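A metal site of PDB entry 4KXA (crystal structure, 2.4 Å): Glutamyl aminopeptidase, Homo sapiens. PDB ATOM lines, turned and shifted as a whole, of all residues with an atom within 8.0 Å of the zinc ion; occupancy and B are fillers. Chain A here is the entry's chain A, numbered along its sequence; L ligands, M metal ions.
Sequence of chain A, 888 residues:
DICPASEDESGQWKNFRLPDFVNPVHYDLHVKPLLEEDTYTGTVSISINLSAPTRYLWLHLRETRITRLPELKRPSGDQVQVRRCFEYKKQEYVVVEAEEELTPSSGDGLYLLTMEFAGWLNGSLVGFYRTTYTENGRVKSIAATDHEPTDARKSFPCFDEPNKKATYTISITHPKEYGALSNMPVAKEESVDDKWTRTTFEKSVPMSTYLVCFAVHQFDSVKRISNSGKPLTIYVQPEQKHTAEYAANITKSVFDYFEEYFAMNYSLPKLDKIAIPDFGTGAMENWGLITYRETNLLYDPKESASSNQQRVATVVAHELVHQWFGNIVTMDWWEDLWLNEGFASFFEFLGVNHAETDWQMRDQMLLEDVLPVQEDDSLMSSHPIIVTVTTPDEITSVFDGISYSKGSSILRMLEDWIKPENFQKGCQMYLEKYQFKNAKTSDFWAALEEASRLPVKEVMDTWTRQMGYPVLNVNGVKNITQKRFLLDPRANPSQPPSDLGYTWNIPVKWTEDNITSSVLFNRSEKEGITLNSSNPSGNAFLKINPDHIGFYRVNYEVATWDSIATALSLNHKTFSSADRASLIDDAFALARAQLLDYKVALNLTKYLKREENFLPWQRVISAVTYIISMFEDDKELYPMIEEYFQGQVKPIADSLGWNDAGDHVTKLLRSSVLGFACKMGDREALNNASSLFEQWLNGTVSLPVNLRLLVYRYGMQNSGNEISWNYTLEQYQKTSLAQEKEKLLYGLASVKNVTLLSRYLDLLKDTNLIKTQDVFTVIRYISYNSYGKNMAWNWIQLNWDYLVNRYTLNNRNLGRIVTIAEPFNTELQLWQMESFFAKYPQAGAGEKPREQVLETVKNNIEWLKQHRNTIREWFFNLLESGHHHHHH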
ATOM      1  N   GLU A 148     -12.084   6.661  -2.662  1.00  0.00           N
ATOM      2  CA  GLU A 148     -10.648   6.879  -2.488  1.00  0.00           C
ATOM      3  C   GLU A 148      -9.825   5.716  -3.052  1.00  0.00           C
ATOM      4  O   GLU A 148     -10.081   4.572  -2.702  1.00  0.00           O
ATOM      5  CB  GLU A 148     -10.290   7.111  -1.011  1.00  0.00           C
ATOM      6  CG  GLU A 148      -8.908   7.718  -0.823  1.00  0.00           C
ATOM      7  CD  GLU A 148      -8.679   8.296   0.572  1.00  0.00           C
ATOM      8  OE1 GLU A 148      -9.189   7.718   1.559  1.00  0.00           O
ATOM      9  OE2 GLU A 148      -7.956   9.309   0.664  1.00  0.00           O
ATOM     10  N   ALA A 283     -12.424   1.561   6.483  1.00  0.00           N
ATOM     11  CA  ALA A 283     -13.324   2.672   6.755  1.00  0.00           C
ATOM     12  C   ALA A 283     -12.947   3.824   5.840  1.00  0.00           C
ATOM     13  O   ALA A 283     -11.830   3.898   5.368  1.00  0.00           O
ATOM     14  CB  ALA A 283     -13.213   3.101   8.207  1.00  0.00           C
ATOM     15  N   MET A 284     -13.894   4.735   5.616  1.00  0.00           N
ATOM     16  CA  MET A 284     -13.667   5.852   4.724  1.00  0.00           C
ATOM     17  C   MET A 284     -14.184   7.163   5.322  1.00  0.00           C
ATOM     18  O   MET A 284     -15.316   7.231   5.803  1.00  0.00           O
ATOM     19  CB  MET A 284     -14.307   5.573   3.358  1.00  0.00           C
ATOM     20  CG  MET A 284     -14.031   6.642   2.331  1.00  0.00           C
ATOM     21  SD  MET A 284     -12.265   6.995   2.258  1.00  0.00           S
ATOM     22  CE  MET A 284     -12.327   8.684   1.676  1.00  0.00           C
ATOM     23  N   GLU A 285     -13.352   8.192   5.265  1.00  0.00           N
ATOM     24  CA  GLU A 285     -13.600   9.445   5.976  1.00  0.00           C
ATOM     25  C   GLU A 285     -14.457  10.464   5.210  1.00  0.00           C
ATOM     26  O   GLU A 285     -14.294  11.687   5.390  1.00  0.00           O
ATOM     27  CB  GLU A 285     -12.276  10.073   6.381  1.00  0.00           C
ATOM     28  CG  GLU A 285     -11.450  10.595   5.217  1.00  0.00           C
ATOM     29  CD  GLU A 285     -10.437   9.603   4.693  1.00  0.00           C
ATOM     30  OE1 GLU A 285     -10.525   8.385   5.003  1.00  0.00           O
ATOM     31  OE2 GLU A 285      -9.536  10.067   3.946  1.00  0.00           O
ATOM     32  N   VAL A 315     -10.178   3.095  14.993  1.00  0.00           N
ATOM     33  CA  VAL A 315     -10.645   3.402  13.634  1.00  0.00           C
ATOM     34  C   VAL A 315     -11.601   4.589  13.657  1.00  0.00           C
ATOM     35  O   VAL A 315     -11.487   5.495  12.836  1.00  0.00           O
ATOM     36  CB  VAL A 315     -11.285   2.196  12.942  1.00  0.00           C
ATOM     37  CG1 VAL A 315     -11.708   2.561  11.534  1.00  0.00           C
ATOM     38  CG2 VAL A 315     -10.291   1.031  12.893  1.00  0.00           C
ATOM     39  N   HIS A 318      -9.420   7.553  14.212  1.00  0.00           N
ATOM     40  CA  HIS A 318      -8.715   7.772  12.945  1.00  0.00           C
ATOM     41  C   HIS A 318      -9.609   8.529  11.968  1.00  0.00           C
ATOM     42  O   HIS A 318      -9.189   9.506  11.359  1.00  0.00           O
ATOM     43  CB  HIS A 318      -8.298   6.409  12.341  1.00  0.00           C
ATOM     44  CG  HIS A 318      -7.478   6.498  11.088  1.00  0.00           C
ATOM     45  ND1 HIS A 318      -6.103   6.369  11.071  1.00  0.00           N
ATOM     46  CD2 HIS A 318      -7.847   6.673   9.790  1.00  0.00           C
ATOM     47  CE1 HIS A 318      -5.659   6.482   9.831  1.00  0.00           C
ATOM     48  NE2 HIS A 318      -6.690   6.659   9.037  1.00  0.00           N
ATOM     49  N   GLU A 319     -10.842   8.065  11.830  1.00  0.00           N
ATOM     50  CA  GLU A 319     -11.782   8.653  10.893  1.00  0.00           C
ATOM     51  C   GLU A 319     -12.145  10.076  11.276  1.00  0.00           C
ATOM     52  O   GLU A 319     -12.394  10.910  10.406  1.00  0.00           O
ATOM     53  CB  GLU A 319     -13.025   7.772  10.754  1.00  0.00           C
ATOM     54  CG  GLU A 319     -12.725   6.385  10.210  1.00  0.00           C
ATOM     55  CD  GLU A 319     -11.808   6.394   8.995  1.00  0.00           C
ATOM     56  OE1 GLU A 319     -12.058   7.176   8.060  1.00  0.00           O
ATOM     57  OE2 GLU A 319     -10.843   5.604   8.963  1.00  0.00           O
ATOM     58  N   VAL A 321     -10.092  12.211  12.936  1.00  0.00           N
ATOM     59  CA  VAL A 321      -8.938  13.057  12.643  1.00  0.00           C
ATOM     60  C   VAL A 321      -9.037  13.606  11.226  1.00  0.00           C
ATOM     61  O   VAL A 321      -8.730  14.768  10.983  1.00  0.00           O
ATOM     62  CB  VAL A 321      -7.602  12.308  12.817  1.00  0.00           C
ATOM     63  CG1 VAL A 321      -6.432  13.241  12.510  1.00  0.00           C
ATOM     64  CG2 VAL A 321      -7.464  11.767  14.214  1.00  0.00           C
ATOM     65  N   HIS A 322      -9.491  12.772  10.310  1.00  0.00           N
ATOM     66  CA  HIS A 322      -9.556  13.130   8.910  1.00  0.00           C
ATOM     67  C   HIS A 322     -10.485  14.305   8.639  1.00  0.00           C
ATOM     68  O   HIS A 322     -10.314  15.038   7.661  1.00  0.00           O
ATOM     69  CB  HIS A 322      -9.987  11.933   8.081  1.00  0.00           C
ATOM     70  CG  HIS A 322      -8.852  11.035   7.675  1.00  0.00           C
ATOM     71  ND1 HIS A 322      -7.762  11.486   6.972  1.00  0.00           N
ATOM     72  CD2 HIS A 322      -8.670   9.702   7.857  1.00  0.00           C
ATOM     73  CE1 HIS A 322      -6.944  10.475   6.740  1.00  0.00           C
ATOM     74  NE2 HIS A 322      -7.472   9.379   7.260  1.00  0.00           N
ATOM     75  N   PHE A 325      -7.673  16.828   9.351  1.00  0.00           N
ATOM     76  CA  PHE A 325      -6.537  16.532   8.482  1.00  0.00           C
ATOM     77  C   PHE A 325      -6.930  15.552   7.384  1.00  0.00           C
ATOM     78  O   PHE A 325      -7.002  14.339   7.595  1.00  0.00           O
ATOM     79  CB  PHE A 325      -5.350  16.012   9.291  1.00  0.00           C
ATOM     80  CG  PHE A 325      -4.695  17.066  10.111  1.00  0.00           C
ATOM     81  CD1 PHE A 325      -3.745  17.916   9.558  1.00  0.00           C
ATOM     82  CD2 PHE A 325      -5.055  17.244  11.445  1.00  0.00           C
ATOM     83  CE1 PHE A 325      -3.150  18.901  10.312  1.00  0.00           C
ATOM     84  CE2 PHE A 325      -4.456  18.237  12.202  1.00  0.00           C
ATOM     85  CZ  PHE A 325      -3.507  19.068  11.638  1.00  0.00           C
ATOM     86  N   LEU A 337       0.323  12.134   0.351  1.00  0.00           N
ATOM     87  CA  LEU A 337      -0.745  11.368   1.037  1.00  0.00           C
ATOM     88  C   LEU A 337      -0.548  11.259   2.557  1.00  0.00           C
ATOM     89  O   LEU A 337      -1.533  11.293   3.304  1.00  0.00           O
ATOM     90  CB  LEU A 337      -0.880   9.955   0.450  1.00  0.00           C
ATOM     91  CG  LEU A 337      -1.827   8.984   1.169  1.00  0.00           C
ATOM     92  CD1 LEU A 337      -3.280   9.452   1.122  1.00  0.00           C
ATOM     93  CD2 LEU A 337      -1.713   7.598   0.572  1.00  0.00           C
ATOM     94  N   ASN A 340      -2.355  13.269   5.133  1.00  0.00           N
ATOM     95  CA  ASN A 340      -3.648  12.783   5.592  1.00  0.00           C
ATOM     96  C   ASN A 340      -3.465  11.612   6.525  1.00  0.00           C
ATOM     97  O   ASN A 340      -3.829  11.681   7.698  1.00  0.00           O
ATOM     98  CB  ASN A 340      -4.538  12.379   4.404  1.00  0.00           C
ATOM     99  CG  ASN A 340      -5.069  13.565   3.605  1.00  0.00           C
ATOM    100  OD1 ASN A 340      -5.834  13.384   2.656  1.00  0.00           O
ATOM    101  ND2 ASN A 340      -4.667  14.779   3.994  1.00  0.00           N
ATOM    102  N   GLU A 341      -2.862  10.548   6.008  1.00  0.00           N
ATOM    103  CA  GLU A 341      -2.822   9.257   6.691  1.00  0.00           C
ATOM    104  C   GLU A 341      -1.896   9.183   7.894  1.00  0.00           C
ATOM    105  O   GLU A 341      -2.241   8.574   8.904  1.00  0.00           O
ATOM    106  CB  GLU A 341      -2.521   8.124   5.702  1.00  0.00           C
ATOM    107  CG  GLU A 341      -3.461   8.080   4.495  1.00  0.00           C
ATOM    108  CD  GLU A 341      -4.929   7.889   4.849  1.00  0.00           C
ATOM    109  OE1 GLU A 341      -5.249   7.499   5.990  1.00  0.00           O
ATOM    110  OE2 GLU A 341      -5.775   8.107   3.975  1.00  0.00           O
ATOM    111  N   GLY A 342      -0.727   9.797   7.776  1.00  0.00           N
ATOM    112  CA  GLY A 342       0.216   9.871   8.893  1.00  0.00           C
ATOM    113  C   GLY A 342      -0.397  10.598  10.075  1.00  0.00           C
ATOM    114  O   GLY A 342      -0.337  10.115  11.202  1.00  0.00           O
ATOM    115  N   PHE A 343      -0.999  11.751   9.796  1.00  0.00           N
ATOM    116  CA  PHE A 343      -1.655  12.571  10.822  1.00  0.00           C
ATOM    117  C   PHE A 343      -2.799  11.838  11.482  1.00  0.00           C
ATOM    118  O   PHE A 343      -2.932  11.870  12.712  1.00  0.00           O
ATOM    119  CB  PHE A 343      -2.155  13.878  10.213  1.00  0.00           C
ATOM    120  CG  PHE A 343      -1.069  14.858   9.932  1.00  0.00           C
ATOM    121  CD1 PHE A 343      -0.075  14.567   8.998  1.00  0.00           C
ATOM    122  CD2 PHE A 343      -1.032  16.074  10.588  1.00  0.00           C
ATOM    123  CE1 PHE A 343       0.944  15.471   8.743  1.00  0.00           C
ATOM    124  CE2 PHE A 343      -0.026  16.985  10.332  1.00  0.00           C
ATOM    125  CZ  PHE A 343       0.962  16.683   9.409  1.00  0.00           C
ATOM    126  N   ALA A 344      -3.635  11.190  10.673  1.00  0.00           N
ATOM    127  CA  ALA A 344      -4.720  10.362  11.179  1.00  0.00           C
ATOM    128  C   ALA A 344      -4.203   9.213  12.046  1.00  0.00           C
ATOM    129  O   ALA A 344      -4.727   8.970  13.136  1.00  0.00           O
ATOM    130  CB  ALA A 344      -5.562   9.832  10.035  1.00  0.00           C
ATOM    131  N   SER A 345      -3.165   8.520  11.554  1.00  0.00           N
ATOM    132  CA  SER A 345      -2.534   7.416  12.284  1.00  0.00           C
ATOM    133  C   SER A 345      -1.847   7.873  13.575  1.00  0.00           C
ATOM    134  O   SER A 345      -1.676   7.075  14.499  1.00  0.00           O
ATOM    135  CB  SER A 345      -1.549   6.629  11.396  1.00  0.00           C
ATOM    136  OG  SER A 345      -2.222   5.864  10.408  1.00  0.00           O
ATOM    137  N   GLU A 348      -4.937   9.415  16.134  1.00  0.00           N
ATOM    138  CA  GLU A 348      -5.851   8.353  16.548  1.00  0.00           C
ATOM    139  C   GLU A 348      -5.534   7.899  17.973  1.00  0.00           C
ATOM    140  O   GLU A 348      -6.443   7.626  18.752  1.00  0.00           O
ATOM    141  CB  GLU A 348      -5.833   7.176  15.567  1.00  0.00           C
ATOM    142  CG  GLU A 348      -4.545   6.366  15.570  1.00  0.00           C
ATOM    143  CD  GLU A 348      -4.552   5.215  14.579  1.00  0.00           C
ATOM    144  OE1 GLU A 348      -3.856   4.204  14.839  1.00  0.00           O
ATOM    145  OE2 GLU A 348      -5.241   5.305  13.537  1.00  0.00           O
ATOM    146  N   PHE A 399      -1.112   3.746  -0.263  1.00  0.00           N
ATOM    147  CA  PHE A 399      -1.871   3.585   0.978  1.00  0.00           C
ATOM    148  C   PHE A 399      -1.278   2.400   1.739  1.00  0.00           C
ATOM    149  O   PHE A 399      -1.848   1.309   1.755  1.00  0.00           O
ATOM    150  CB  PHE A 399      -3.359   3.376   0.684  1.00  0.00           C
ATOM    151  CG  PHE A 399      -4.050   4.612   0.194  1.00  0.00           C
ATOM    152  CD1 PHE A 399      -4.029   4.948  -1.155  1.00  0.00           C
ATOM    153  CD2 PHE A 399      -4.714   5.457   1.083  1.00  0.00           C
ATOM    154  CE1 PHE A 399      -4.651   6.108  -1.612  1.00  0.00           C
ATOM    155  CE2 PHE A 399      -5.340   6.615   0.639  1.00  0.00           C
ATOM    156  CZ  PHE A 399      -5.310   6.937  -0.709  1.00  0.00           C
ATOM    157  N   TYR A 404       1.051   5.437   6.437  1.00  0.00           N
ATOM    158  CA  TYR A 404       0.387   5.364   7.732  1.00  0.00           C
ATOM    159  C   TYR A 404       1.382   5.302   8.884  1.00  0.00           C
ATOM    160  O   TYR A 404       1.460   6.235   9.685  1.00  0.00           O
ATOM    161  CB  TYR A 404      -0.540   4.141   7.794  1.00  0.00           C
ATOM    162  CG  TYR A 404      -1.827   4.262   6.997  1.00  0.00           C
ATOM    163  CD1 TYR A 404      -1.820   4.148   5.606  1.00  0.00           C
ATOM    164  CD2 TYR A 404      -3.042   4.471   7.634  1.00  0.00           C
ATOM    165  CE1 TYR A 404      -2.998   4.245   4.872  1.00  0.00           C
ATOM    166  CE2 TYR A 404      -4.221   4.573   6.930  1.00  0.00           C
ATOM    167  CZ  TYR A 404      -4.198   4.461   5.542  1.00  0.00           C
ATOM    168  OH  TYR A 404      -5.377   4.564   4.838  1.00  0.00           O
HETATM  169  N1  LIG L   1      -8.755   5.959   3.520  1.00  0.00           N
HETATM  170  C1  LIG L   1      -9.070   4.508   3.700  1.00  0.00           C
HETATM  171  C2  LIG L   1      -8.734   3.992   5.105  1.00  0.00           C
HETATM  172  O1  LIG L   1      -9.322   3.028   5.579  1.00  0.00           O
HETATM  173  C3  LIG L   1      -8.343   3.661   2.641  1.00  0.00           C
HETATM  174  C4  LIG L   1      -9.147   3.501   1.352  1.00  0.00           C
HETATM  175  O2  LIG L   1     -10.399   3.498   1.427  1.00  0.00           O
HETATM  176  O3  LIG L   1      -8.522   3.372   0.269  1.00  0.00           O
HETATM  177  O4  LIG L   1      -7.876   4.530   5.802  1.00  0.00           O
HETATM  178 ZN    ZN M   1      -7.047   7.219   6.773  1.00  0.00          ZN
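A nitrogen (N1) of the ligand is in salt-bridge range of the side-chain carboxylate (OE2) of Glu 341.
The side-chain hydroxyl of Tyr 404 lies within hydrogen-bond range of an oxygen (O4) of the ligand.
The side-chain carboxylate of Glu 285 is in salt-bridge range of a nitrogen (N1) of the ligand (3.3 Å).
OE1 of Glu 148 is in salt-bridge range of N1 of the ligand (2.7 Å).
The backbone carbonyl oxygen (O) of Ala 283 lies close to an oxygen (O1) of the ligand, 2.7 Å away.
The side-chain carboxylate (OE1) of Glu 341 sits close to the side-chain hydroxyl (OH) of Tyr 404 (3.2 Å).
The backbone carbonyl oxygen of Glu 341 lies within hydrogen-bond range of the side-chain hydroxyl of Ser 345, 3.1 Å away.
The backbone carbonyl oxygen (O) of Phe 325 sits at hydrogen-bond distance from a ring nitrogen (ND1) of His 322 (3.0 Å).
The side-chain carboxylate (OE2) of Glu 348 is in hydrogen-bond range of a ring nitrogen (ND1) of His 318 (2.8 Å).
Merely in contact with the zinc ion: Tyr 404.
Of the 20 residues printed, 4 come within 4 Å of the zinc ion.
The nearest printed residue that does not touch the zinc ion is Glu 285 (4.1 Å).
The zinc ion is bound by the side-chain carboxylate of Glu 341 (2.0 Å), a ring nitrogen (NE2) of His 322 (2.3 Å) and a ring nitrogen (NE2) of His 318 (2.4 Å).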
